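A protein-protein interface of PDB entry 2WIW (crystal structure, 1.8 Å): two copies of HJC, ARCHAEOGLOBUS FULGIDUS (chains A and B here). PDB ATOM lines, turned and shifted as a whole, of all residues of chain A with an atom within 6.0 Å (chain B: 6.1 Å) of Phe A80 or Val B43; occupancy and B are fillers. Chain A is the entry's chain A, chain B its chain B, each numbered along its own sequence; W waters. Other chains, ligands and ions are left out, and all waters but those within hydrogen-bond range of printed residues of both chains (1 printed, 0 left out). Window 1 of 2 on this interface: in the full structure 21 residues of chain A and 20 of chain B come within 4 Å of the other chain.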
ATOM      1  N   ILE A  27       8.897 -26.433 -15.628  1.00  0.00           N
ATOM      2  CA  ILE A  27       8.165 -25.425 -16.365  1.00  0.00           C
ATOM      3  C   ILE A  27       8.668 -24.017 -16.076  1.00  0.00           C
ATOM      4  O   ILE A  27       9.170 -23.730 -14.984  1.00  0.00           O
ATOM      5  CB  ILE A  27       6.648 -25.507 -16.096  1.00  0.00           C
ATOM      6  CG1 ILE A  27       6.345 -25.355 -14.614  1.00  0.00           C
ATOM      7  CG2 ILE A  27       6.104 -26.847 -16.607  1.00  0.00           C
ATOM      8  CD1 ILE A  27       5.980 -23.951 -14.195  1.00  0.00           C
ATOM      9  N   VAL A  43       9.682 -23.759 -12.064  1.00  0.00           N
ATOM     10  CA  VAL A  43       9.296 -24.707 -11.029  1.00  0.00           C
ATOM     11  C   VAL A  43       9.537 -26.116 -11.553  1.00  0.00           C
ATOM     12  O   VAL A  43       9.175 -26.426 -12.693  1.00  0.00           O
ATOM     13  CB  VAL A  43       7.802 -24.515 -10.630  1.00  0.00           C
ATOM     14  CG1 VAL A  43       7.373 -25.613  -9.698  1.00  0.00           C
ATOM     15  CG2 VAL A  43       7.633 -23.144  -9.968  1.00  0.00           C
ATOM     16  N   ALA A  44      10.138 -26.976 -10.744  1.00  0.00           N
ATOM     17  CA  ALA A  44      10.486 -28.299 -11.248  1.00  0.00           C
ATOM     18  C   ALA A  44      10.200 -29.367 -10.234  1.00  0.00           C
ATOM     19  O   ALA A  44      10.218 -29.105  -9.035  1.00  0.00           O
ATOM     20  CB  ALA A  44      11.989 -28.321 -11.678  1.00  0.00           C
ATOM     21  N   TYR A  50      11.092 -31.108  -5.075  1.00  0.00           N
ATOM     22  CA  TYR A  50      10.443 -30.019  -5.823  1.00  0.00           C
ATOM     23  C   TYR A  50      11.273 -28.761  -5.679  1.00  0.00           C
ATOM     24  O   TYR A  50      11.720 -28.458  -4.570  1.00  0.00           O
ATOM     25  CB  TYR A  50       9.050 -29.740  -5.259  1.00  0.00           C
ATOM     26  CG  TYR A  50       8.145 -30.941  -5.395  1.00  0.00           C
ATOM     27  CD1 TYR A  50       7.359 -31.123  -6.521  1.00  0.00           C
ATOM     28  CD2 TYR A  50       8.109 -31.901  -4.397  1.00  0.00           C
ATOM     29  CE1 TYR A  50       6.528 -32.257  -6.647  1.00  0.00           C
ATOM     30  CE2 TYR A  50       7.291 -33.032  -4.504  1.00  0.00           C
ATOM     31  CZ  TYR A  50       6.507 -33.201  -5.622  1.00  0.00           C
ATOM     32  OH  TYR A  50       5.712 -34.336  -5.679  1.00  0.00           O
ATOM     33  N   THR A  75       8.715 -17.329   0.259  1.00  0.00           N
ATOM     34  CA  THR A  75       7.293 -17.410   0.590  1.00  0.00           C
ATOM     35  C   THR A  75       6.611 -18.350  -0.389  1.00  0.00           C
ATOM     36  O   THR A  75       5.792 -19.175  -0.006  1.00  0.00           O
ATOM     37  CB  THR A  75       6.644 -16.024   0.560  1.00  0.00           C
ATOM     38  OG1 THR A  75       7.234 -15.218   1.596  1.00  0.00           O
ATOM     39  CG2 THR A  75       5.126 -16.110   0.795  1.00  0.00           C
ATOM     40  N   PHE A  76       6.972 -18.242  -1.658  1.00  0.00           N
ATOM     41  CA  PHE A  76       6.397 -19.140  -2.656  1.00  0.00           C
ATOM     42  C   PHE A  76       6.779 -20.583  -2.338  1.00  0.00           C
ATOM     43  O   PHE A  76       5.942 -21.495  -2.330  1.00  0.00           O
ATOM     44  CB  PHE A  76       6.874 -18.791  -4.067  1.00  0.00           C
ATOM     45  CG  PHE A  76       6.449 -19.806  -5.064  1.00  0.00           C
ATOM     46  CD1 PHE A  76       5.204 -19.704  -5.682  1.00  0.00           C
ATOM     47  CD2 PHE A  76       7.247 -20.909  -5.320  1.00  0.00           C
ATOM     48  CE1 PHE A  76       4.778 -20.682  -6.583  1.00  0.00           C
ATOM     49  CE2 PHE A  76       6.823 -21.897  -6.229  1.00  0.00           C
ATOM     50  CZ  PHE A  76       5.580 -21.773  -6.849  1.00  0.00           C
ATOM     51  N   ALA A  77       8.069 -20.810  -2.121  1.00  0.00           N
ATOM     52  CA  ALA A  77       8.564 -22.146  -1.856  1.00  0.00           C
ATOM     53  C   ALA A  77       7.834 -22.772  -0.659  1.00  0.00           C
ATOM     54  O   ALA A  77       7.448 -23.929  -0.699  1.00  0.00           O
ATOM     55  CB  ALA A  77      10.088 -22.125  -1.632  1.00  0.00           C
ATOM     56  N   ARG A  78       7.657 -22.012   0.417  1.00  0.00           N
ATOM     57  CA  ARG A  78       6.963 -22.538   1.588  1.00  0.00           C
ATOM     58  C   ARG A  78       5.479 -22.850   1.269  1.00  0.00           C
ATOM     59  O   ARG A  78       4.930 -23.875   1.708  1.00  0.00           O
ATOM     60  CB  ARG A  78       7.055 -21.522   2.744  1.00  0.00           C
ATOM     61  CG  ARG A  78       6.329 -21.965   4.004  1.00  0.00           C
ATOM     62  CD  ARG A  78       6.736 -21.132   5.225  1.00  0.00           C
ATOM     63  NE  ARG A  78       8.158 -21.269   5.553  1.00  0.00           N
ATOM     64  CZ  ARG A  78       9.056 -20.285   5.493  1.00  0.00           C
ATOM     65  NH1 ARG A  78       8.702 -19.056   5.130  1.00  0.00           N
ATOM     66  NH2 ARG A  78      10.319 -20.531   5.817  1.00  0.00           N
ATOM     67  N   GLY A  79       4.830 -21.966   0.522  1.00  0.00           N
ATOM     68  CA  GLY A  79       3.402 -22.133   0.236  1.00  0.00           C
ATOM     69  C   GLY A  79       3.177 -23.258  -0.752  1.00  0.00           C
ATOM     70  O   GLY A  79       2.147 -23.936  -0.703  1.00  0.00           O
ATOM     71  N   PHE A  80       4.152 -23.478  -1.630  1.00  0.00           N
ATOM     72  CA  PHE A  80       4.030 -24.497  -2.686  1.00  0.00           C
ATOM     73  C   PHE A  80       4.425 -25.891  -2.199  1.00  0.00           C
ATOM     74  O   PHE A  80       3.814 -26.879  -2.598  1.00  0.00           O
ATOM     75  CB  PHE A  80       4.899 -24.116  -3.884  1.00  0.00           C
ATOM     76  CG  PHE A  80       4.726 -25.034  -5.088  1.00  0.00           C
ATOM     77  CD1 PHE A  80       3.807 -24.709  -6.082  1.00  0.00           C
ATOM     78  CD2 PHE A  80       5.470 -26.195  -5.208  1.00  0.00           C
ATOM     79  CE1 PHE A  80       3.632 -25.549  -7.208  1.00  0.00           C
ATOM     80  CE2 PHE A  80       5.305 -27.047  -6.327  1.00  0.00           C
ATOM     81  CZ  PHE A  80       4.376 -26.721  -7.310  1.00  0.00           C
ATOM     82  N   GLY A  81       5.421 -25.958  -1.307  1.00  0.00           N
ATOM     83  CA  GLY A  81       6.044 -27.220  -0.920  1.00  0.00           C
ATOM     84  C   GLY A  81       7.279 -27.533  -1.776  1.00  0.00           C
ATOM     85  O   GLY A  81       7.472 -28.647  -2.271  1.00  0.00           O
ATOM     86  N   ALA A  82       8.131 -26.532  -1.946  1.00  0.00           N
ATOM     87  CA  ALA A  82       9.335 -26.687  -2.765  1.00  0.00           C
ATOM     88  C   ALA A  82      10.544 -26.124  -2.023  1.00  0.00           C
ATOM     89  O   ALA A  82      10.410 -25.409  -1.025  1.00  0.00           O
ATOM     90  CB  ALA A  82       9.177 -25.967  -4.093  1.00  0.00           C
ATOM     91  N   ALA B  25      -0.334 -22.043  -3.638  1.00  0.00           N
ATOM     92  CA  ALA B  25       0.608 -21.259  -4.423  1.00  0.00           C
ATOM     93  C   ALA B  25       0.524 -21.827  -5.827  1.00  0.00           C
ATOM     94  O   ALA B  25       0.921 -22.975  -6.063  1.00  0.00           O
ATOM     95  CB  ALA B  25       2.038 -21.406  -3.850  1.00  0.00           C
ATOM     96  N   ALA B  26      -0.068 -21.056  -6.731  1.00  0.00           N
ATOM     97  CA  ALA B  26      -0.377 -21.546  -8.090  1.00  0.00           C
ATOM     98  C   ALA B  26       0.295 -20.657  -9.130  1.00  0.00           C
ATOM     99  O   ALA B  26       0.500 -19.454  -8.911  1.00  0.00           O
ATOM    100  CB  ALA B  26      -1.873 -21.567  -8.322  1.00  0.00           C
ATOM    101  N   ILE B  27       0.652 -21.249 -10.260  1.00  0.00           N
ATOM    102  CA  ILE B  27       1.279 -20.480 -11.322  1.00  0.00           C
ATOM    103  C   ILE B  27       0.757 -20.938 -12.693  1.00  0.00           C
ATOM    104  O   ILE B  27       0.449 -22.112 -12.906  1.00  0.00           O
ATOM    105  CB  ILE B  27       2.824 -20.504 -11.261  1.00  0.00           C
ATOM    106  CG1 ILE B  27       3.348 -21.924 -11.276  1.00  0.00           C
ATOM    107  CG2 ILE B  27       3.355 -19.766 -10.010  1.00  0.00           C
ATOM    108  CD1 ILE B  27       3.712 -22.383 -12.650  1.00  0.00           C
ATOM    109  N   ARG B  28       0.574 -19.962 -13.563  1.00  0.00           N
ATOM    110  CA  ARG B  28       0.291 -20.204 -14.977  1.00  0.00           C
ATOM    111  C   ARG B  28       1.603 -20.584 -15.674  1.00  0.00           C
ATOM    112  O   ARG B  28       2.637 -20.004 -15.405  1.00  0.00           O
ATOM    113  CB  ARG B  28      -0.329 -18.937 -15.583  1.00  0.00           C
ATOM    114  CG  ARG B  28      -0.709 -19.021 -17.053  1.00  0.00           C
ATOM    115  CD  ARG B  28      -1.715 -20.127 -17.319  1.00  0.00           C
ATOM    116  NE  ARG B  28      -2.031 -20.270 -18.743  1.00  0.00           N
ATOM    117  CZ  ARG B  28      -1.372 -21.059 -19.592  1.00  0.00           C
ATOM    118  NH1 ARG B  28      -0.348 -21.784 -19.177  1.00  0.00           N
ATOM    119  NH2 ARG B  28      -1.739 -21.125 -20.867  1.00  0.00           N
ATOM    120  N   VAL B  29       1.556 -21.587 -16.544  1.00  0.00           N
ATOM    121  CA  VAL B  29       2.748 -22.084 -17.238  1.00  0.00           C
ATOM    122  C   VAL B  29       2.953 -21.290 -18.527  1.00  0.00           C
ATOM    123  O   VAL B  29       2.018 -21.072 -19.291  1.00  0.00           O
ATOM    124  CB  VAL B  29       2.599 -23.612 -17.568  1.00  0.00           C
ATOM    125  CG1 VAL B  29       3.777 -24.136 -18.390  1.00  0.00           C
ATOM    126  CG2 VAL B  29       2.412 -24.428 -16.294  1.00  0.00           C
ATOM    127  N   PRO B  40       1.121 -28.612 -18.517  1.00  0.00           N
ATOM    128  CA  PRO B  40      -0.246 -28.253 -18.145  1.00  0.00           C
ATOM    129  C   PRO B  40      -0.467 -26.754 -18.247  1.00  0.00           C
ATOM    130  O   PRO B  40       0.464 -26.004 -18.549  1.00  0.00           O
ATOM    131  CB  PRO B  40      -0.333 -28.735 -16.695  1.00  0.00           C
ATOM    132  CG  PRO B  40       1.035 -28.441 -16.154  1.00  0.00           C
ATOM    133  CD  PRO B  40       1.992 -28.723 -17.326  1.00  0.00           C
ATOM    134  N   ASP B  41      -1.689 -26.306 -17.995  1.00  0.00           N
ATOM    135  CA  ASP B  41      -1.959 -24.871 -17.980  1.00  0.00           C
ATOM    136  C   ASP B  41      -1.533 -24.241 -16.669  1.00  0.00           C
ATOM    137  O   ASP B  41      -1.032 -23.106 -16.658  1.00  0.00           O
ATOM    138  CB  ASP B  41      -3.447 -24.609 -18.188  1.00  0.00           C
ATOM    139  CG  ASP B  41      -3.905 -24.977 -19.594  1.00  0.00           C
ATOM    140  OD1 ASP B  41      -3.128 -24.782 -20.556  1.00  0.00           O
ATOM    141  OD2 ASP B  41      -5.038 -25.472 -19.730  1.00  0.00           O
ATOM    142  N   ILE B  42      -1.806 -24.930 -15.570  1.00  0.00           N
ATOM    143  CA  ILE B  42      -1.471 -24.409 -14.236  1.00  0.00           C
ATOM    144  C   ILE B  42      -0.838 -25.514 -13.407  1.00  0.00           C
ATOM    145  O   ILE B  42      -1.146 -26.700 -13.562  1.00  0.00           O
ATOM    146  CB  ILE B  42      -2.720 -23.852 -13.519  1.00  0.00           C
ATOM    147  CG1 ILE B  42      -3.231 -22.582 -14.222  1.00  0.00           C
ATOM    148  CG2 ILE B  42      -2.438 -23.546 -12.033  1.00  0.00           C
ATOM    149  CD1 ILE B  42      -4.569 -22.087 -13.627  1.00  0.00           C
ATOM    150  N   VAL B  43       0.107 -25.140 -12.558  1.00  0.00           N
ATOM    151  CA  VAL B  43       0.649 -26.074 -11.605  1.00  0.00           C
ATOM    152  C   VAL B  43       0.476 -25.412 -10.238  1.00  0.00           C
ATOM    153  O   VAL B  43       0.690 -24.221 -10.110  1.00  0.00           O
ATOM    154  CB  VAL B  43       2.149 -26.349 -11.884  1.00  0.00           C
ATOM    155  CG1 VAL B  43       2.738 -27.187 -10.776  1.00  0.00           C
ATOM    156  CG2 VAL B  43       2.288 -27.063 -13.223  1.00  0.00           C
ATOM    157  N   ALA B  44       0.061 -26.181  -9.242  1.00  0.00           N
ATOM    158  CA  ALA B  44      -0.239 -25.598  -7.913  1.00  0.00           C
ATOM    159  C   ALA B  44       0.214 -26.502  -6.766  1.00  0.00           C
ATOM    160  O   ALA B  44       0.256 -27.708  -6.912  1.00  0.00           O
ATOM    161  CB  ALA B  44      -1.770 -25.319  -7.790  1.00  0.00           C
ATOM    162  N   GLY B  45       0.560 -25.920  -5.608  1.00  0.00           N
ATOM    163  CA  GLY B  45       0.883 -26.735  -4.465  1.00  0.00           C
ATOM    164  C   GLY B  45       0.399 -26.007  -3.223  1.00  0.00           C
ATOM    165  O   GLY B  45       0.275 -24.793  -3.245  1.00  0.00           O
ATOM    166  N   ASN B  46       0.146 -26.732  -2.148  1.00  0.00           N
ATOM    167  CA  ASN B  46      -0.215 -26.032  -0.881  1.00  0.00           C
ATOM    168  C   ASN B  46       0.670 -26.443   0.287  1.00  0.00           C
ATOM    169  O   ASN B  46       0.389 -26.148   1.456  1.00  0.00           O
ATOM    170  CB  ASN B  46      -1.705 -26.241  -0.548  1.00  0.00           C
ATOM    171  CG  ASN B  46      -2.071 -27.699  -0.378  1.00  0.00           C
ATOM    172  OD1 ASN B  46      -1.215 -28.559  -0.254  1.00  0.00           O
ATOM    173  ND2 ASN B  46      -3.363 -27.965  -0.291  1.00  0.00           N
ATOM    174  N   GLY B  47       1.754 -27.125  -0.036  1.00  0.00           N
ATOM    175  CA  GLY B  47       2.683 -27.615   0.956  1.00  0.00           C
ATOM    176  C   GLY B  47       2.602 -29.117   1.133  1.00  0.00           C
ATOM    177  O   GLY B  47       3.586 -29.743   1.546  1.00  0.00           O
ATOM    178  N   ARG B  48       1.432 -29.692   0.831  1.00  0.00           N
ATOM    179  CA  ARG B  48       1.231 -31.143   0.936  1.00  0.00           C
ATOM    180  C   ARG B  48       0.657 -31.791  -0.338  1.00  0.00           C
ATOM    181  O   ARG B  48       0.986 -32.930  -0.648  1.00  0.00           O
ATOM    182  CB  ARG B  48       0.337 -31.472   2.142  1.00  0.00           C
ATOM    183  CG  ARG B  48       1.008 -31.102   3.494  1.00  0.00           C
ATOM    184  CD  ARG B  48       0.174 -31.529   4.687  1.00  0.00           C
ATOM    185  NE  ARG B  48      -0.094 -32.967   4.681  1.00  0.00           N
ATOM    186  CZ  ARG B  48       0.665 -33.877   5.292  1.00  0.00           C
ATOM    187  NH1 ARG B  48       1.748 -33.500   5.961  1.00  0.00           N
ATOM    188  NH2 ARG B  48       0.337 -35.164   5.241  1.00  0.00           N
ATOM    189  N   THR B  49      -0.198 -31.060  -1.045  1.00  0.00           N
ATOM    190  CA  THR B  49      -0.827 -31.516  -2.279  1.00  0.00           C
ATOM    191  C   THR B  49      -0.229 -30.785  -3.482  1.00  0.00           C
ATOM    192  O   THR B  49      -0.016 -29.560  -3.410  1.00  0.00           O
ATOM    193  CB  THR B  49      -2.334 -31.184  -2.262  1.00  0.00           C
ATOM    194  OG1 THR B  49      -2.944 -31.782  -1.113  1.00  0.00           O
ATOM    195  CG2 THR B  49      -3.017 -31.724  -3.545  1.00  0.00           C
ATOM    196  N   TYR B  50       0.014 -31.512  -4.580  1.00  0.00           N
ATOM    197  CA  TYR B  50       0.487 -30.905  -5.819  1.00  0.00           C
ATOM    198  C   TYR B  50      -0.496 -31.210  -6.970  1.00  0.00           C
ATOM    199  O   TYR B  50      -0.898 -32.354  -7.133  1.00  0.00           O
ATOM    200  CB  TYR B  50       1.884 -31.434  -6.181  1.00  0.00           C
ATOM    201  CG  TYR B  50       2.928 -31.213  -5.097  1.00  0.00           C
ATOM    202  CD1 TYR B  50       3.667 -30.033  -5.030  1.00  0.00           C
ATOM    203  CD2 TYR B  50       3.144 -32.180  -4.126  1.00  0.00           C
ATOM    204  CE1 TYR B  50       4.654 -29.851  -4.014  1.00  0.00           C
ATOM    205  CE2 TYR B  50       4.100 -32.002  -3.108  1.00  0.00           C
ATOM    206  CZ  TYR B  50       4.855 -30.834  -3.070  1.00  0.00           C
ATOM    207  OH  TYR B  50       5.777 -30.687  -2.052  1.00  0.00           O
ATOM    208  N   LEU B  51      -0.866 -30.181  -7.727  1.00  0.00           N
ATOM    209  CA  LEU B  51      -1.833 -30.289  -8.834  1.00  0.00           C
ATOM    210  C   LEU B  51      -1.230 -29.881 -10.179  1.00  0.00           C
ATOM    211  O   LEU B  51      -0.556 -28.856 -10.285  1.00  0.00           O
ATOM    212  CB  LEU B  51      -3.007 -29.344  -8.607  1.00  0.00           C
ATOM    213  CG  LEU B  51      -3.662 -29.372  -7.217  1.00  0.00           C
ATOM    214  CD1 LEU B  51      -4.836 -28.376  -7.173  1.00  0.00           C
ATOM    215  CD2 LEU B  51      -4.138 -30.785  -6.899  1.00  0.00           C
ATOM    216  N   ALA B  52      -1.499 -30.678 -11.207  1.00  0.00           N
ATOM    217  CA  ALA B  52      -1.233 -30.298 -12.589  1.00  0.00           C
ATOM    218  C   ALA B  52      -2.587 -30.181 -13.244  1.00  0.00           C
ATOM    219  O   ALA B  52      -3.361 -31.171 -13.237  1.00  0.00           O
ATOM    220  CB  ALA B  52      -0.395 -31.368 -13.283  1.00  0.00           C
ATOM    221  N   ILE B  53      -2.893 -28.995 -13.778  1.00  0.00           N
ATOM    222  CA  ILE B  53      -4.283 -28.688 -14.199  1.00  0.00           C
ATOM    223  C   ILE B  53      -4.371 -28.249 -15.653  1.00  0.00           C
ATOM    224  O   ILE B  53      -3.656 -27.364 -16.092  1.00  0.00           O
ATOM    225  CB  ILE B  53      -4.900 -27.554 -13.328  1.00  0.00           C
ATOM    226  CG1 ILE B  53      -4.768 -27.903 -11.849  1.00  0.00           C
ATOM    227  CG2 ILE B  53      -6.381 -27.339 -13.683  1.00  0.00           C
ATOM    228  CD1 ILE B  53      -4.988 -26.691 -10.920  1.00  0.00           C
ATOM    229  N   PHE B  76       2.939 -35.645 -17.707  1.00  0.00           N
ATOM    230  CA  PHE B  76       3.563 -34.534 -16.957  1.00  0.00           C
ATOM    231  C   PHE B  76       3.388 -34.741 -15.465  1.00  0.00           C
ATOM    232  O   PHE B  76       4.342 -34.638 -14.677  1.00  0.00           O
ATOM    233  CB  PHE B  76       2.955 -33.180 -17.301  1.00  0.00           C
ATOM    234  CG  PHE B  76       3.528 -32.048 -16.454  1.00  0.00           C
ATOM    235  CD1 PHE B  76       4.718 -31.442 -16.817  1.00  0.00           C
ATOM    236  CD2 PHE B  76       2.897 -31.645 -15.276  1.00  0.00           C
ATOM    237  CE1 PHE B  76       5.262 -30.423 -16.036  1.00  0.00           C
ATOM    238  CE2 PHE B  76       3.445 -30.627 -14.479  1.00  0.00           C
ATOM    239  CZ  PHE B  76       4.616 -30.010 -14.874  1.00  0.00           C
ATOM    240  N   PHE B  80       6.444 -35.033 -12.787  1.00  0.00           N
ATOM    241  CA  PHE B  80       6.596 -33.923 -11.832  1.00  0.00           C
ATOM    242  C   PHE B  80       6.324 -34.400 -10.403  1.00  0.00           C
ATOM    243  O   PHE B  80       7.020 -33.992  -9.471  1.00  0.00           O
ATOM    244  CB  PHE B  80       5.669 -32.778 -12.233  1.00  0.00           C
ATOM    245  CG  PHE B  80       5.789 -31.534 -11.364  1.00  0.00           C
ATOM    246  CD1 PHE B  80       6.588 -30.460 -11.770  1.00  0.00           C
ATOM    247  CD2 PHE B  80       5.076 -31.421 -10.172  1.00  0.00           C
ATOM    248  CE1 PHE B  80       6.678 -29.301 -10.988  1.00  0.00           C
ATOM    249  CE2 PHE B  80       5.181 -30.278  -9.380  1.00  0.00           C
ATOM    250  CZ  PHE B  80       5.975 -29.225  -9.777  1.00  0.00           C
ATOM    251  N   ALA B  82       2.655 -34.833  -9.293  1.00  0.00           N
ATOM    252  CA  ALA B  82       1.450 -34.076  -9.018  1.00  0.00           C
ATOM    253  C   ALA B  82       0.248 -34.941  -9.384  1.00  0.00           C
ATOM    254  O   ALA B  82       0.398 -35.950 -10.075  1.00  0.00           O
ATOM    255  CB  ALA B  82       1.409 -32.837  -9.837  1.00  0.00           C
HETATM  256  O   HOH W   1       2.630 -29.165  -1.726  1.00  0.00           O
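Phe A80 touches just these residues of chain B: Ala B25 (3.4 Å), Val B43 (3.9 Å), Ala B44 (3.6 Å), Gly B45 (3.5 Å), Asn B46 (3.7 Å), Gly B47 (3.3 Å), Tyr B50 (3.4 Å) and Phe B80 (3.9 Å).
Of the printed residues of chain A, Val B43 touches Phe A80 (3.9 Å).
Of the printed residues of chain A, Val B29 touches Ile A27.
Printed residues of chain B within 4 Å of Gly A79: Ala B25, Gly B45, Asn B46 and Gly B47.
Of the printed residues of chain A, Gly B47 touches Gly A79, Phe A80 and Gly A81.
Of the printed residues of chain A, Ala B44 touches Phe A80.
Ile B42 touches none of the printed residues of chain A.
The nearest residue of chain B that does not touch Phe A80 is Thr B49 (4.7 Å).
The nearest printed residue of chain B that does not touch Phe A76 is Ala B26 (4.9 Å).
N of Ile A27 lies within hydrogen-bond range of O of Val A43 (2.9 Å).
N of Ala B25 is in hydrogen-bond range of O of Gly B45 (2.8 Å).
The backbone carbonyl oxygen of Val B43 is in hydrogen-bond range of the backbone NH of Ile B27 (3.0 Å).
The backbone NH of Val B29 lies within hydrogen-bond range of the backbone carbonyl oxygen of Asp B41, at 3.0 Å.
The backbone carbonyl oxygen of Ala B44 is in hydrogen-bond range of the backbone NH of Leu B51 (2.8 Å).
OD1 of Asn B46 lies within hydrogen-bond range of N of Thr B49, at 2.8 Å.
Hydrophobic or aromatic side chains of chain A that line the printed part of chain B: Ile A27, Val A43, Tyr A50, Phe A76 and Phe A80.
Among the printed residues, 23 pairs touch across the chains.
N of Gly B47 lies within hydrogen-bond range of O of Gly A79 (3.3 Å).
N of Gly B47 lies within hydrogen-bond range of O of Phe A80 (3.3 Å).
The side-chain hydroxyl (OH) of Tyr B50 sits at hydrogen-bond distance from the backbone carbonyl oxygen (O) of Gly A81 (2.7 Å).
O of Gly B45 lies close to O of Gly A79 (3.3 Å).
Ile A27 touches Phe B76, and with the chains exchanged Phe A76 touches Ile B27.
Val A43 touches Phe B80, and with the chains exchanged Phe A80 touches Val B43.
Ala A44 touches Phe B80, and with the chains exchanged Phe A80 touches Ala B44.
Tyr A50 touches Phe B80, and with the chains exchanged Phe A80 touches Tyr B50.
Of the 23 pairs that touch across the chains among the printed residues, 11 have their exchanged pair printed and touching as well.
Water W1 lies within hydrogen-bond range of O of Phe A80 (2.7 Å), N of Gly B47 (2.8 Å), N of Arg B48 (2.9 Å) and O of Thr B49 (3.2 Å).
CZ of Phe B80 touches CG1 of Val A43, 3.9 Å away.
Tyr B50 touches Tyr A50 (OH to CD2, 3.5 Å).
Tyr A50 touches Phe B80.
Phe A76 touches Ile B27.
Ala B25 touches Gly A79.
Gly A79 touches Asn B46 (O to C, 3.1 Å).
Phe A80 touches Ala B44.
Phe A80 touches Gly B45 (O to CA, 3.5 Å).
Phe A80 touches Asn B46 (O to N, 3.7 Å).
Phe A80 touches Tyr B50 (O to CE1, 3.4 Å).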
